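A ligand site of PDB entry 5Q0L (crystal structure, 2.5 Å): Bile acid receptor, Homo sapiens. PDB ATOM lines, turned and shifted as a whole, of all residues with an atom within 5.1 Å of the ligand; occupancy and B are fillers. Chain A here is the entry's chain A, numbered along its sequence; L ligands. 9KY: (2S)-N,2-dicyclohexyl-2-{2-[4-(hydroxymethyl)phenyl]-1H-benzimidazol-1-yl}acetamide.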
ATOM      1  N   ILE A  30       8.061  25.761 -19.152  1.00  0.00           N
ATOM      2  CA  ILE A  30       8.962  24.602 -19.241  1.00  0.00           C
ATOM      3  C   ILE A  30       8.167  23.278 -19.155  1.00  0.00           C
ATOM      4  O   ILE A  30       8.294  22.436 -20.050  1.00  0.00           O
ATOM      5  CB  ILE A  30      10.101  24.732 -18.185  1.00  0.00           C
ATOM      6  CG1 ILE A  30      10.993  25.955 -18.481  1.00  0.00           C
ATOM      7  CG2 ILE A  30      10.946  23.459 -18.090  1.00  0.00           C
ATOM      8  CD1 ILE A  30      10.864  27.103 -17.546  1.00  0.00           C
ATOM      9  N   ILE A  34       7.209  20.096 -22.085  1.00  0.00           N
ATOM     10  CA  ILE A  34       7.654  18.702 -22.023  1.00  0.00           C
ATOM     11  C   ILE A  34       6.489  17.734 -21.648  1.00  0.00           C
ATOM     12  O   ILE A  34       6.555  16.561 -22.014  1.00  0.00           O
ATOM     13  CB  ILE A  34       8.937  18.498 -21.151  1.00  0.00           C
ATOM     14  CG1 ILE A  34       8.628  18.209 -19.687  1.00  0.00           C
ATOM     15  CG2 ILE A  34       9.932  19.667 -21.274  1.00  0.00           C
ATOM     16  CD1 ILE A  34       9.446  17.060 -19.140  1.00  0.00           C
ATOM     17  N   ASN A  44      15.132  16.670 -27.035  1.00  0.00           N
ATOM     18  CA  ASN A  44      15.286  16.947 -25.613  1.00  0.00           C
ATOM     19  C   ASN A  44      16.644  17.618 -25.291  1.00  0.00           C
ATOM     20  O   ASN A  44      16.693  18.513 -24.446  1.00  0.00           O
ATOM     21  CB  ASN A  44      15.085  15.668 -24.793  1.00  0.00           C
ATOM     22  CG  ASN A  44      13.646  15.285 -24.584  1.00  0.00           C
ATOM     23  OD1 ASN A  44      12.757  16.124 -24.391  1.00  0.00           O
ATOM     24  ND2 ASN A  44      13.395  13.986 -24.557  1.00  0.00           N
ATOM     25  N   ILE A  47      16.171  21.056 -26.557  1.00  0.00           N
ATOM     26  CA  ILE A  47      15.307  21.780 -25.609  1.00  0.00           C
ATOM     27  C   ILE A  47      16.165  22.263 -24.439  1.00  0.00           C
ATOM     28  O   ILE A  47      16.156  23.461 -24.160  1.00  0.00           O
ATOM     29  CB  ILE A  47      14.049  20.962 -25.141  1.00  0.00           C
ATOM     30  CG1 ILE A  47      13.033  20.783 -26.287  1.00  0.00           C
ATOM     31  CG2 ILE A  47      13.357  21.649 -23.929  1.00  0.00           C
ATOM     32  CD1 ILE A  47      12.098  19.593 -26.163  1.00  0.00           C
ATOM     33  N   LEU A  48      16.962  21.358 -23.804  1.00  0.00           N
ATOM     34  CA  LEU A  48      17.826  21.707 -22.688  1.00  0.00           C
ATOM     35  C   LEU A  48      18.825  22.827 -23.032  1.00  0.00           C
ATOM     36  O   LEU A  48      18.913  23.805 -22.290  1.00  0.00           O
ATOM     37  CB  LEU A  48      18.538  20.454 -22.115  1.00  0.00           C
ATOM     38  CG  LEU A  48      19.718  20.686 -21.147  1.00  0.00           C
ATOM     39  CD1 LEU A  48      19.250  21.210 -19.788  1.00  0.00           C
ATOM     40  CD2 LEU A  48      20.573  19.445 -21.035  1.00  0.00           C
ATOM     41  N   MET A  51      16.922  26.119 -23.307  1.00  0.00           N
ATOM     42  CA  MET A  51      16.528  26.420 -21.929  1.00  0.00           C
ATOM     43  C   MET A  51      17.692  27.020 -21.131  1.00  0.00           C
ATOM     44  O   MET A  51      17.513  28.051 -20.480  1.00  0.00           O
ATOM     45  CB  MET A  51      16.049  25.138 -21.219  1.00  0.00           C
ATOM     46  CG  MET A  51      14.713  24.635 -21.694  1.00  0.00           C
ATOM     47  SD  MET A  51      13.326  25.910 -21.359  1.00  0.00           S
ATOM     48  CE  MET A  51      11.858  24.990 -22.179  1.00  0.00           C
ATOM     49  N   ALA A  52      18.865  26.363 -21.198  1.00  0.00           N
ATOM     50  CA  ALA A  52      20.091  26.713 -20.494  1.00  0.00           C
ATOM     51  C   ALA A  52      20.729  28.005 -20.991  1.00  0.00           C
ATOM     52  O   ALA A  52      21.346  28.718 -20.190  1.00  0.00           O
ATOM     53  CB  ALA A  52      21.080  25.569 -20.587  1.00  0.00           C
ATOM     54  N   HIS A  55      18.492  30.658 -19.606  1.00  0.00           N
ATOM     55  CA  HIS A  55      18.814  30.663 -18.191  1.00  0.00           C
ATOM     56  C   HIS A  55      20.093  31.454 -17.879  1.00  0.00           C
ATOM     57  O   HIS A  55      20.046  32.305 -17.004  1.00  0.00           O
ATOM     58  CB  HIS A  55      18.916  29.227 -17.614  1.00  0.00           C
ATOM     59  CG  HIS A  55      19.378  29.206 -16.199  1.00  0.00           C
ATOM     60  ND1 HIS A  55      18.516  29.533 -15.157  1.00  0.00           N
ATOM     61  CD2 HIS A  55      20.612  28.989 -15.680  1.00  0.00           C
ATOM     62  CE1 HIS A  55      19.254  29.478 -14.059  1.00  0.00           C
ATOM     63  NE2 HIS A  55      20.512  29.179 -14.332  1.00  0.00           N
ATOM     64  N   MET A  89      21.313  26.697 -12.257  1.00  0.00           N
ATOM     65  CA  MET A  89      20.522  25.973 -13.239  1.00  0.00           C
ATOM     66  C   MET A  89      19.811  24.761 -12.573  1.00  0.00           C
ATOM     67  O   MET A  89      18.595  24.624 -12.736  1.00  0.00           O
ATOM     68  CB  MET A  89      21.472  25.545 -14.356  1.00  0.00           C
ATOM     69  CG  MET A  89      20.801  25.140 -15.630  1.00  0.00           C
ATOM     70  SD  MET A  89      21.195  23.285 -16.079  1.00  0.00           S
ATOM     71  CE  MET A  89      23.188  23.320 -15.907  1.00  0.00           C
ATOM     72  N   PHE A  90      20.552  23.909 -11.823  1.00  0.00           N
ATOM     73  CA  PHE A  90      19.976  22.761 -11.132  1.00  0.00           C
ATOM     74  C   PHE A  90      19.045  23.175 -10.007  1.00  0.00           C
ATOM     75  O   PHE A  90      18.056  22.480  -9.764  1.00  0.00           O
ATOM     76  CB  PHE A  90      21.057  21.781 -10.633  1.00  0.00           C
ATOM     77  CG  PHE A  90      21.578  20.851 -11.704  1.00  0.00           C
ATOM     78  CD1 PHE A  90      20.806  19.804 -12.177  1.00  0.00           C
ATOM     79  CD2 PHE A  90      22.837  21.033 -12.252  1.00  0.00           C
ATOM     80  CE1 PHE A  90      21.277  18.960 -13.175  1.00  0.00           C
ATOM     81  CE2 PHE A  90      23.324  20.166 -13.236  1.00  0.00           C
ATOM     82  CZ  PHE A  90      22.539  19.132 -13.696  1.00  0.00           C
ATOM     83  N   ARG A  92      17.163  25.906 -10.105  1.00  0.00           N
ATOM     84  CA  ARG A  92      16.004  26.393 -10.860  1.00  0.00           C
ATOM     85  C   ARG A  92      15.185  25.220 -11.388  1.00  0.00           C
ATOM     86  O   ARG A  92      13.951  25.294 -11.392  1.00  0.00           O
ATOM     87  CB  ARG A  92      16.454  27.319 -11.993  1.00  0.00           C
ATOM     88  CG  ARG A  92      15.327  27.993 -12.783  1.00  0.00           C
ATOM     89  CD  ARG A  92      14.488  28.928 -11.936  1.00  0.00           C
ATOM     90  NE  ARG A  92      13.317  29.386 -12.684  1.00  0.00           N
ATOM     91  CZ  ARG A  92      12.225  29.898 -12.142  1.00  0.00           C
ATOM     92  NH1 ARG A  92      12.139  30.047 -10.832  1.00  0.00           N
ATOM     93  NH2 ARG A  92      11.217  30.277 -12.904  1.00  0.00           N
ATOM     94  N   SER A  93      15.855  24.130 -11.844  1.00  0.00           N
ATOM     95  CA  SER A  93      15.205  22.900 -12.326  1.00  0.00           C
ATOM     96  C   SER A  93      14.510  22.241 -11.158  1.00  0.00           C
ATOM     97  O   SER A  93      13.373  21.787 -11.312  1.00  0.00           O
ATOM     98  CB  SER A  93      16.233  21.931 -12.895  1.00  0.00           C
ATOM     99  OG  SER A  93      16.977  22.492 -13.952  1.00  0.00           O
ATOM    100  N   ALA A  94      15.175  22.225  -9.979  1.00  0.00           N
ATOM    101  CA  ALA A  94      14.650  21.683  -8.718  1.00  0.00           C
ATOM    102  C   ALA A  94      13.418  22.490  -8.277  1.00  0.00           C
ATOM    103  O   ALA A  94      12.415  21.893  -7.900  1.00  0.00           O
ATOM    104  CB  ALA A  94      15.725  21.742  -7.636  1.00  0.00           C
ATOM    105  N   ILE A  96      11.357  24.290 -10.348  1.00  0.00           N
ATOM    106  CA  ILE A  96      10.371  23.945 -11.367  1.00  0.00           C
ATOM    107  C   ILE A  96       9.782  22.553 -11.129  1.00  0.00           C
ATOM    108  O   ILE A  96       8.553  22.412 -11.082  1.00  0.00           O
ATOM    109  CB  ILE A  96      10.941  24.118 -12.807  1.00  0.00           C
ATOM    110  CG1 ILE A  96      11.243  25.621 -13.114  1.00  0.00           C
ATOM    111  CG2 ILE A  96      10.000  23.509 -13.870  1.00  0.00           C
ATOM    112  CD1 ILE A  96      12.191  25.874 -14.276  1.00  0.00           C
ATOM    113  N   PHE A  97      10.649  21.542 -10.952  1.00  0.00           N
ATOM    114  CA  PHE A  97      10.241  20.142 -10.719  1.00  0.00           C
ATOM    115  C   PHE A  97       9.247  20.007  -9.571  1.00  0.00           C
ATOM    116  O   PHE A  97       8.261  19.272  -9.696  1.00  0.00           O
ATOM    117  CB  PHE A  97      11.483  19.277 -10.482  1.00  0.00           C
ATOM    118  CG  PHE A  97      11.235  17.789 -10.342  1.00  0.00           C
ATOM    119  CD1 PHE A  97      11.127  16.978 -11.467  1.00  0.00           C
ATOM    120  CD2 PHE A  97      11.136  17.192  -9.082  1.00  0.00           C
ATOM    121  CE1 PHE A  97      10.882  15.614 -11.343  1.00  0.00           C
ATOM    122  CE2 PHE A  97      10.912  15.822  -8.954  1.00  0.00           C
ATOM    123  CZ  PHE A  97      10.796  15.045 -10.090  1.00  0.00           C
ATOM    124  N   LEU A 109       6.058  14.227 -15.666  1.00  0.00           N
ATOM    125  CA  LEU A 109       7.190  15.139 -15.809  1.00  0.00           C
ATOM    126  C   LEU A 109       8.479  14.405 -15.448  1.00  0.00           C
ATOM    127  O   LEU A 109       9.442  14.429 -16.210  1.00  0.00           O
ATOM    128  CB  LEU A 109       6.971  16.380 -14.915  1.00  0.00           C
ATOM    129  CG  LEU A 109       8.088  17.454 -14.879  1.00  0.00           C
ATOM    130  CD1 LEU A 109       8.039  18.342 -16.091  1.00  0.00           C
ATOM    131  CD2 LEU A 109       7.978  18.324 -13.645  1.00  0.00           C
ATOM    132  N   ARG A 112       9.292  11.695 -17.918  1.00  0.00           N
ATOM    133  CA  ARG A 112       9.757  12.349 -19.148  1.00  0.00           C
ATOM    134  C   ARG A 112      11.210  12.826 -19.032  1.00  0.00           C
ATOM    135  O   ARG A 112      11.933  12.739 -20.021  1.00  0.00           O
ATOM    136  CB  ARG A 112       8.808  13.478 -19.584  1.00  0.00           C
ATOM    137  CG  ARG A 112       8.075  13.172 -20.892  1.00  0.00           C
ATOM    138  CD  ARG A 112       6.630  12.784 -20.655  1.00  0.00           C
ATOM    139  NE  ARG A 112       6.005  12.168 -21.827  1.00  0.00           N
ATOM    140  CZ  ARG A 112       4.870  12.588 -22.374  1.00  0.00           C
ATOM    141  NH1 ARG A 112       4.239  13.645 -21.888  1.00  0.00           N
ATOM    142  NH2 ARG A 112       4.353  11.951 -23.413  1.00  0.00           N
ATOM    143  N   ILE A 113      11.641  13.277 -17.823  1.00  0.00           N
ATOM    144  CA  ILE A 113      13.041  13.670 -17.573  1.00  0.00           C
ATOM    145  C   ILE A 113      13.909  12.393 -17.513  1.00  0.00           C
ATOM    146  O   ILE A 113      15.038  12.380 -17.996  1.00  0.00           O
ATOM    147  CB  ILE A 113      13.227  14.569 -16.297  1.00  0.00           C
ATOM    148  CG1 ILE A 113      12.419  15.884 -16.381  1.00  0.00           C
ATOM    149  CG2 ILE A 113      14.717  14.891 -16.051  1.00  0.00           C
ATOM    150  CD1 ILE A 113      12.116  16.526 -15.072  1.00  0.00           C
ATOM    151  N   SER A 116      14.489  11.206 -21.020  1.00  0.00           N
ATOM    152  CA  SER A 116      14.805  12.347 -21.876  1.00  0.00           C
ATOM    153  C   SER A 116      16.004  12.084 -22.793  1.00  0.00           C
ATOM    154  O   SER A 116      15.996  12.524 -23.932  1.00  0.00           O
ATOM    155  CB  SER A 116      15.059  13.590 -21.043  1.00  0.00           C
ATOM    156  OG  SER A 116      16.193  13.413 -20.214  1.00  0.00           O
ATOM    157  N   ILE A 118      19.441  11.390 -20.903  1.00  0.00           N
ATOM    158  CA  ILE A 118      20.577  11.361 -19.971  1.00  0.00           C
ATOM    159  C   ILE A 118      20.860   9.923 -19.533  1.00  0.00           C
ATOM    160  O   ILE A 118      19.963   9.076 -19.548  1.00  0.00           O
ATOM    161  CB  ILE A 118      20.330  12.263 -18.704  1.00  0.00           C
ATOM    162  CG1 ILE A 118      19.373  13.432 -18.997  1.00  0.00           C
ATOM    163  CG2 ILE A 118      21.646  12.762 -18.084  1.00  0.00           C
ATOM    164  CD1 ILE A 118      18.478  13.789 -17.843  1.00  0.00           C
ATOM    165  N   MET A 126      20.422  13.348  -9.314  1.00  0.00           N
ATOM    166  CA  MET A 126      19.632  14.491  -9.753  1.00  0.00           C
ATOM    167  C   MET A 126      18.231  14.471  -9.142  1.00  0.00           C
ATOM    168  O   MET A 126      17.791  15.495  -8.618  1.00  0.00           O
ATOM    169  CB  MET A 126      19.530  14.477 -11.276  1.00  0.00           C
ATOM    170  CG  MET A 126      19.327  15.835 -11.900  1.00  0.00           C
ATOM    171  SD  MET A 126      18.424  15.683 -13.642  1.00  0.00           S
ATOM    172  CE  MET A 126      19.389  14.105 -14.366  1.00  0.00           C
ATOM    173  N   TYR A 130      16.435  16.781  -6.220  1.00  0.00           N
ATOM    174  CA  TYR A 130      15.131  17.422  -6.462  1.00  0.00           C
ATOM    175  C   TYR A 130      14.140  17.116  -5.352  1.00  0.00           C
ATOM    176  O   TYR A 130      13.587  18.041  -4.754  1.00  0.00           O
ATOM    177  CB  TYR A 130      14.534  17.007  -7.829  1.00  0.00           C
ATOM    178  CG  TYR A 130      15.257  17.515  -9.069  1.00  0.00           C
ATOM    179  CD1 TYR A 130      16.268  18.462  -8.962  1.00  0.00           C
ATOM    180  CD2 TYR A 130      14.922  17.055 -10.334  1.00  0.00           C
ATOM    181  CE1 TYR A 130      16.941  18.924 -10.085  1.00  0.00           C
ATOM    182  CE2 TYR A 130      15.575  17.506 -11.466  1.00  0.00           C
ATOM    183  CZ  TYR A 130      16.589  18.444 -11.333  1.00  0.00           C
ATOM    184  OH  TYR A 130      17.269  18.888 -12.440  1.00  0.00           O
ATOM    185  N   HIS A 208      29.279  17.715 -14.400  1.00  0.00           N
ATOM    186  CA  HIS A 208      28.380  18.292 -15.396  1.00  0.00           C
ATOM    187  C   HIS A 208      28.775  18.044 -16.870  1.00  0.00           C
ATOM    188  O   HIS A 208      27.911  17.649 -17.654  1.00  0.00           O
ATOM    189  CB  HIS A 208      28.148  19.792 -15.155  1.00  0.00           C
ATOM    190  CG  HIS A 208      27.043  20.340 -15.999  1.00  0.00           C
ATOM    191  ND1 HIS A 208      25.774  19.790 -15.986  1.00  0.00           N
ATOM    192  CD2 HIS A 208      27.063  21.331 -16.917  1.00  0.00           C
ATOM    193  CE1 HIS A 208      25.061  20.474 -16.858  1.00  0.00           C
ATOM    194  NE2 HIS A 208      25.788  21.427 -17.436  1.00  0.00           N
ATOM    195  N   MET A 211      27.949  14.607 -17.711  1.00  0.00           N
ATOM    196  CA  MET A 211      26.479  14.470 -17.782  1.00  0.00           C
ATOM    197  C   MET A 211      25.974  14.796 -19.184  1.00  0.00           C
ATOM    198  O   MET A 211      25.143  14.071 -19.726  1.00  0.00           O
ATOM    199  CB  MET A 211      25.770  15.420 -16.792  1.00  0.00           C
ATOM    200  CG  MET A 211      25.665  14.887 -15.388  1.00  0.00           C
ATOM    201  SD  MET A 211      24.269  15.782 -14.290  1.00  0.00           S
ATOM    202  CE  MET A 211      22.681  15.272 -15.353  1.00  0.00           C
ATOM    203  N   LEU A 212      26.473  15.927 -19.745  1.00  0.00           N
ATOM    204  CA  LEU A 212      26.101  16.438 -21.065  1.00  0.00           C
ATOM    205  C   LEU A 212      26.582  15.533 -22.198  1.00  0.00           C
ATOM    206  O   LEU A 212      25.787  15.240 -23.096  1.00  0.00           O
ATOM    207  CB  LEU A 212      26.637  17.844 -21.270  1.00  0.00           C
ATOM    208  CG  LEU A 212      26.217  18.910 -20.260  1.00  0.00           C
ATOM    209  CD1 LEU A 212      27.203  20.038 -20.253  1.00  0.00           C
ATOM    210  CD2 LEU A 212      24.787  19.378 -20.498  1.00  0.00           C
ATOM    211  N   TRP A 215      24.582  12.174 -22.800  1.00  0.00           N
ATOM    212  CA  TRP A 215      23.265  12.241 -23.453  1.00  0.00           C
ATOM    213  C   TRP A 215      23.279  11.345 -24.688  1.00  0.00           C
ATOM    214  O   TRP A 215      24.235  11.387 -25.467  1.00  0.00           O
ATOM    215  CB  TRP A 215      22.920  13.675 -23.894  1.00  0.00           C
ATOM    216  CG  TRP A 215      22.055  14.427 -22.921  1.00  0.00           C
ATOM    217  CD1 TRP A 215      22.470  15.125 -21.820  1.00  0.00           C
ATOM    218  CD2 TRP A 215      20.650  14.655 -23.035  1.00  0.00           C
ATOM    219  NE1 TRP A 215      21.391  15.740 -21.220  1.00  0.00           N
ATOM    220  CE2 TRP A 215      20.255  15.458 -21.938  1.00  0.00           C
ATOM    221  CE3 TRP A 215      19.659  14.249 -23.954  1.00  0.00           C
ATOM    222  CZ2 TRP A 215      18.927  15.850 -21.717  1.00  0.00           C
ATOM    223  CZ3 TRP A 215      18.352  14.635 -23.729  1.00  0.00           C
ATOM    224  CH2 TRP A 215      18.000  15.427 -22.626  1.00  0.00           C
HETATM  225  N3  9KY L   1      15.674  19.039 -14.761  1.00  0.00           N
HETATM  226  C4  9KY L   1      15.547  21.727 -18.462  1.00  0.00           C
HETATM  227  C5  9KY L   1      15.729  20.222 -18.257  1.00  0.00           C
HETATM  228  C6  9KY L   1      14.162  20.107 -16.120  1.00  0.00           C
HETATM  229  C7  9KY L   1      14.385  19.583 -14.850  1.00  0.00           C
HETATM  230  C13 9KY L   1      17.909  17.631 -16.919  1.00  0.00           C
HETATM  231  C15 9KY L   1      19.895  19.456 -16.335  1.00  0.00           C
HETATM  232  C17 9KY L   1      20.249  18.269 -16.938  1.00  0.00           C
HETATM  233  C21 9KY L   1      21.685  17.977 -17.256  1.00  0.00           C
HETATM  234  C22 9KY L   1      14.172  18.234 -18.834  1.00  0.00           C
HETATM  235  C24 9KY L   1      17.637  24.438 -17.322  1.00  0.00           C
HETATM  236  C26 9KY L   1      11.950  20.764 -15.477  1.00  0.00           C
HETATM  237  C28 9KY L   1      14.621  18.708 -21.752  1.00  0.00           C
HETATM  238  C1  9KY L   1      16.203  19.226 -15.958  1.00  0.00           C
HETATM  239  N2  9KY L   1      15.360  19.861 -16.827  1.00  0.00           N
HETATM  240  O10 9KY L   1      14.837  22.182 -19.347  1.00  0.00           O
HETATM  241  N8  9KY L   1      16.218  22.479 -17.586  1.00  0.00           N
HETATM  242  C14 9KY L   1      16.207  23.940 -17.561  1.00  0.00           C
HETATM  243  C31 9KY L   1      17.684  25.953 -17.193  1.00  0.00           C
HETATM  244  C32 9KY L   1      16.765  26.441 -16.081  1.00  0.00           C
HETATM  245  C30 9KY L   1      15.323  25.973 -16.338  1.00  0.00           C
HETATM  246  C25 9KY L   1      15.260  24.451 -16.468  1.00  0.00           C
HETATM  247  C11 9KY L   1      15.262  19.186 -19.321  1.00  0.00           C
HETATM  248  C29 9KY L   1      13.972  17.077 -19.839  1.00  0.00           C
HETATM  249  C33 9KY L   1      13.598  17.603 -21.235  1.00  0.00           C
HETATM  250  C23 9KY L   1      14.864  19.814 -20.664  1.00  0.00           C
HETATM  251  C19 9KY L   1      13.387  19.647 -13.880  1.00  0.00           C
HETATM  252  C27 9KY L   1      12.173  20.240 -14.208  1.00  0.00           C
HETATM  253  C18 9KY L   1      12.955  20.700 -16.463  1.00  0.00           C
HETATM  254  C9  9KY L   1      17.574  18.829 -16.307  1.00  0.00           C
HETATM  255  C12 9KY L   1      18.583  19.745 -16.031  1.00  0.00           C
HETATM  256  C16 9KY L   1      19.235  17.354 -17.236  1.00  0.00           C
HETATM  257  O20 9KY L   1      21.828  16.973 -18.247  1.00  0.00           O
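The side-chain sulfur of Met 126 is in hydrogen-bond range of the side-chain hydroxyl of Tyr 130, 3.6 Å away.
The backbone carbonyl oxygen of Met 89 sits at hydrogen-bond distance from the side-chain hydroxyl of Ser 93 (2.9 Å).
The side-chain amide nitrogen of Asn 44 sits at hydrogen-bond distance from the backbone carbonyl oxygen of Ser 116.
A ring nitrogen (NE2) of His 55 is in hydrogen-bond range of the backbone NH of Met 89 (3.3 Å).
The backbone carbonyl oxygen (O) of Ile 113 sits at hydrogen-bond distance from the side-chain hydroxyl (OG) of Ser 116 (2.7 Å).
Ile 30 touches the ligand (CG2 to C18, 3.8 Å).
Asn 44 touches the ligand.
CG2 of Ile 47 touches C28 of the ligand, at 3.9 Å.
Leu 48 touches the ligand.
CG of Met 51 touches O10 of the ligand, at 3.4 Å.
His 55 touches the ligand (CB to C31, 3.5 Å).
Met 89 touches the ligand (CG to C31, 3.6 Å).
Phe 90 touches the ligand (CE1 to C15, 3.5 Å).
Arg 92 touches the ligand.
O of Ser 93 touches C19 of the ligand, at 3.3 Å.
Ile 96 touches the ligand.
Phe 97 touches the ligand.
CD1 of Ile 113 touches C19 of the ligand, 3.6 Å away.
Ser 116 touches the ligand.
Ile 118 touches the ligand.
Met 126 touches the ligand.
Met 211 touches the ligand.
Hydrophobic or aromatic side chains within 4 Å of the ligand: Ile 30, Ile 47, Leu 48, Met 51, His 55, Met 89, Phe 90, Ile 96, Phe 97, Ile 113, Ile 118, Met 126, Tyr 130 and Met 211.
19 residues have an atom within 4 Å of the ligand: Ile 30, Asn 44, Ile 47, Leu 48, Met 51, His 55, Met 89, Phe 90, Arg 92, Ser 93, Ile 96, Phe 97, Ile 113, Ser 116, Ile 118, Met 126, Tyr 130, Met 211 and Trp 215.
Along chain A the residues within 4 Å of the ligand span positions 30 to 215.
N3 of the ligand sits at hydrogen-bond distance from OH of Tyr 130, at 2.8 Å.
The indole nitrogen (NE1) of Trp 215 is in hydrogen-bond range of an oxygen (O20) of the ligand, 3.2 Å away.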
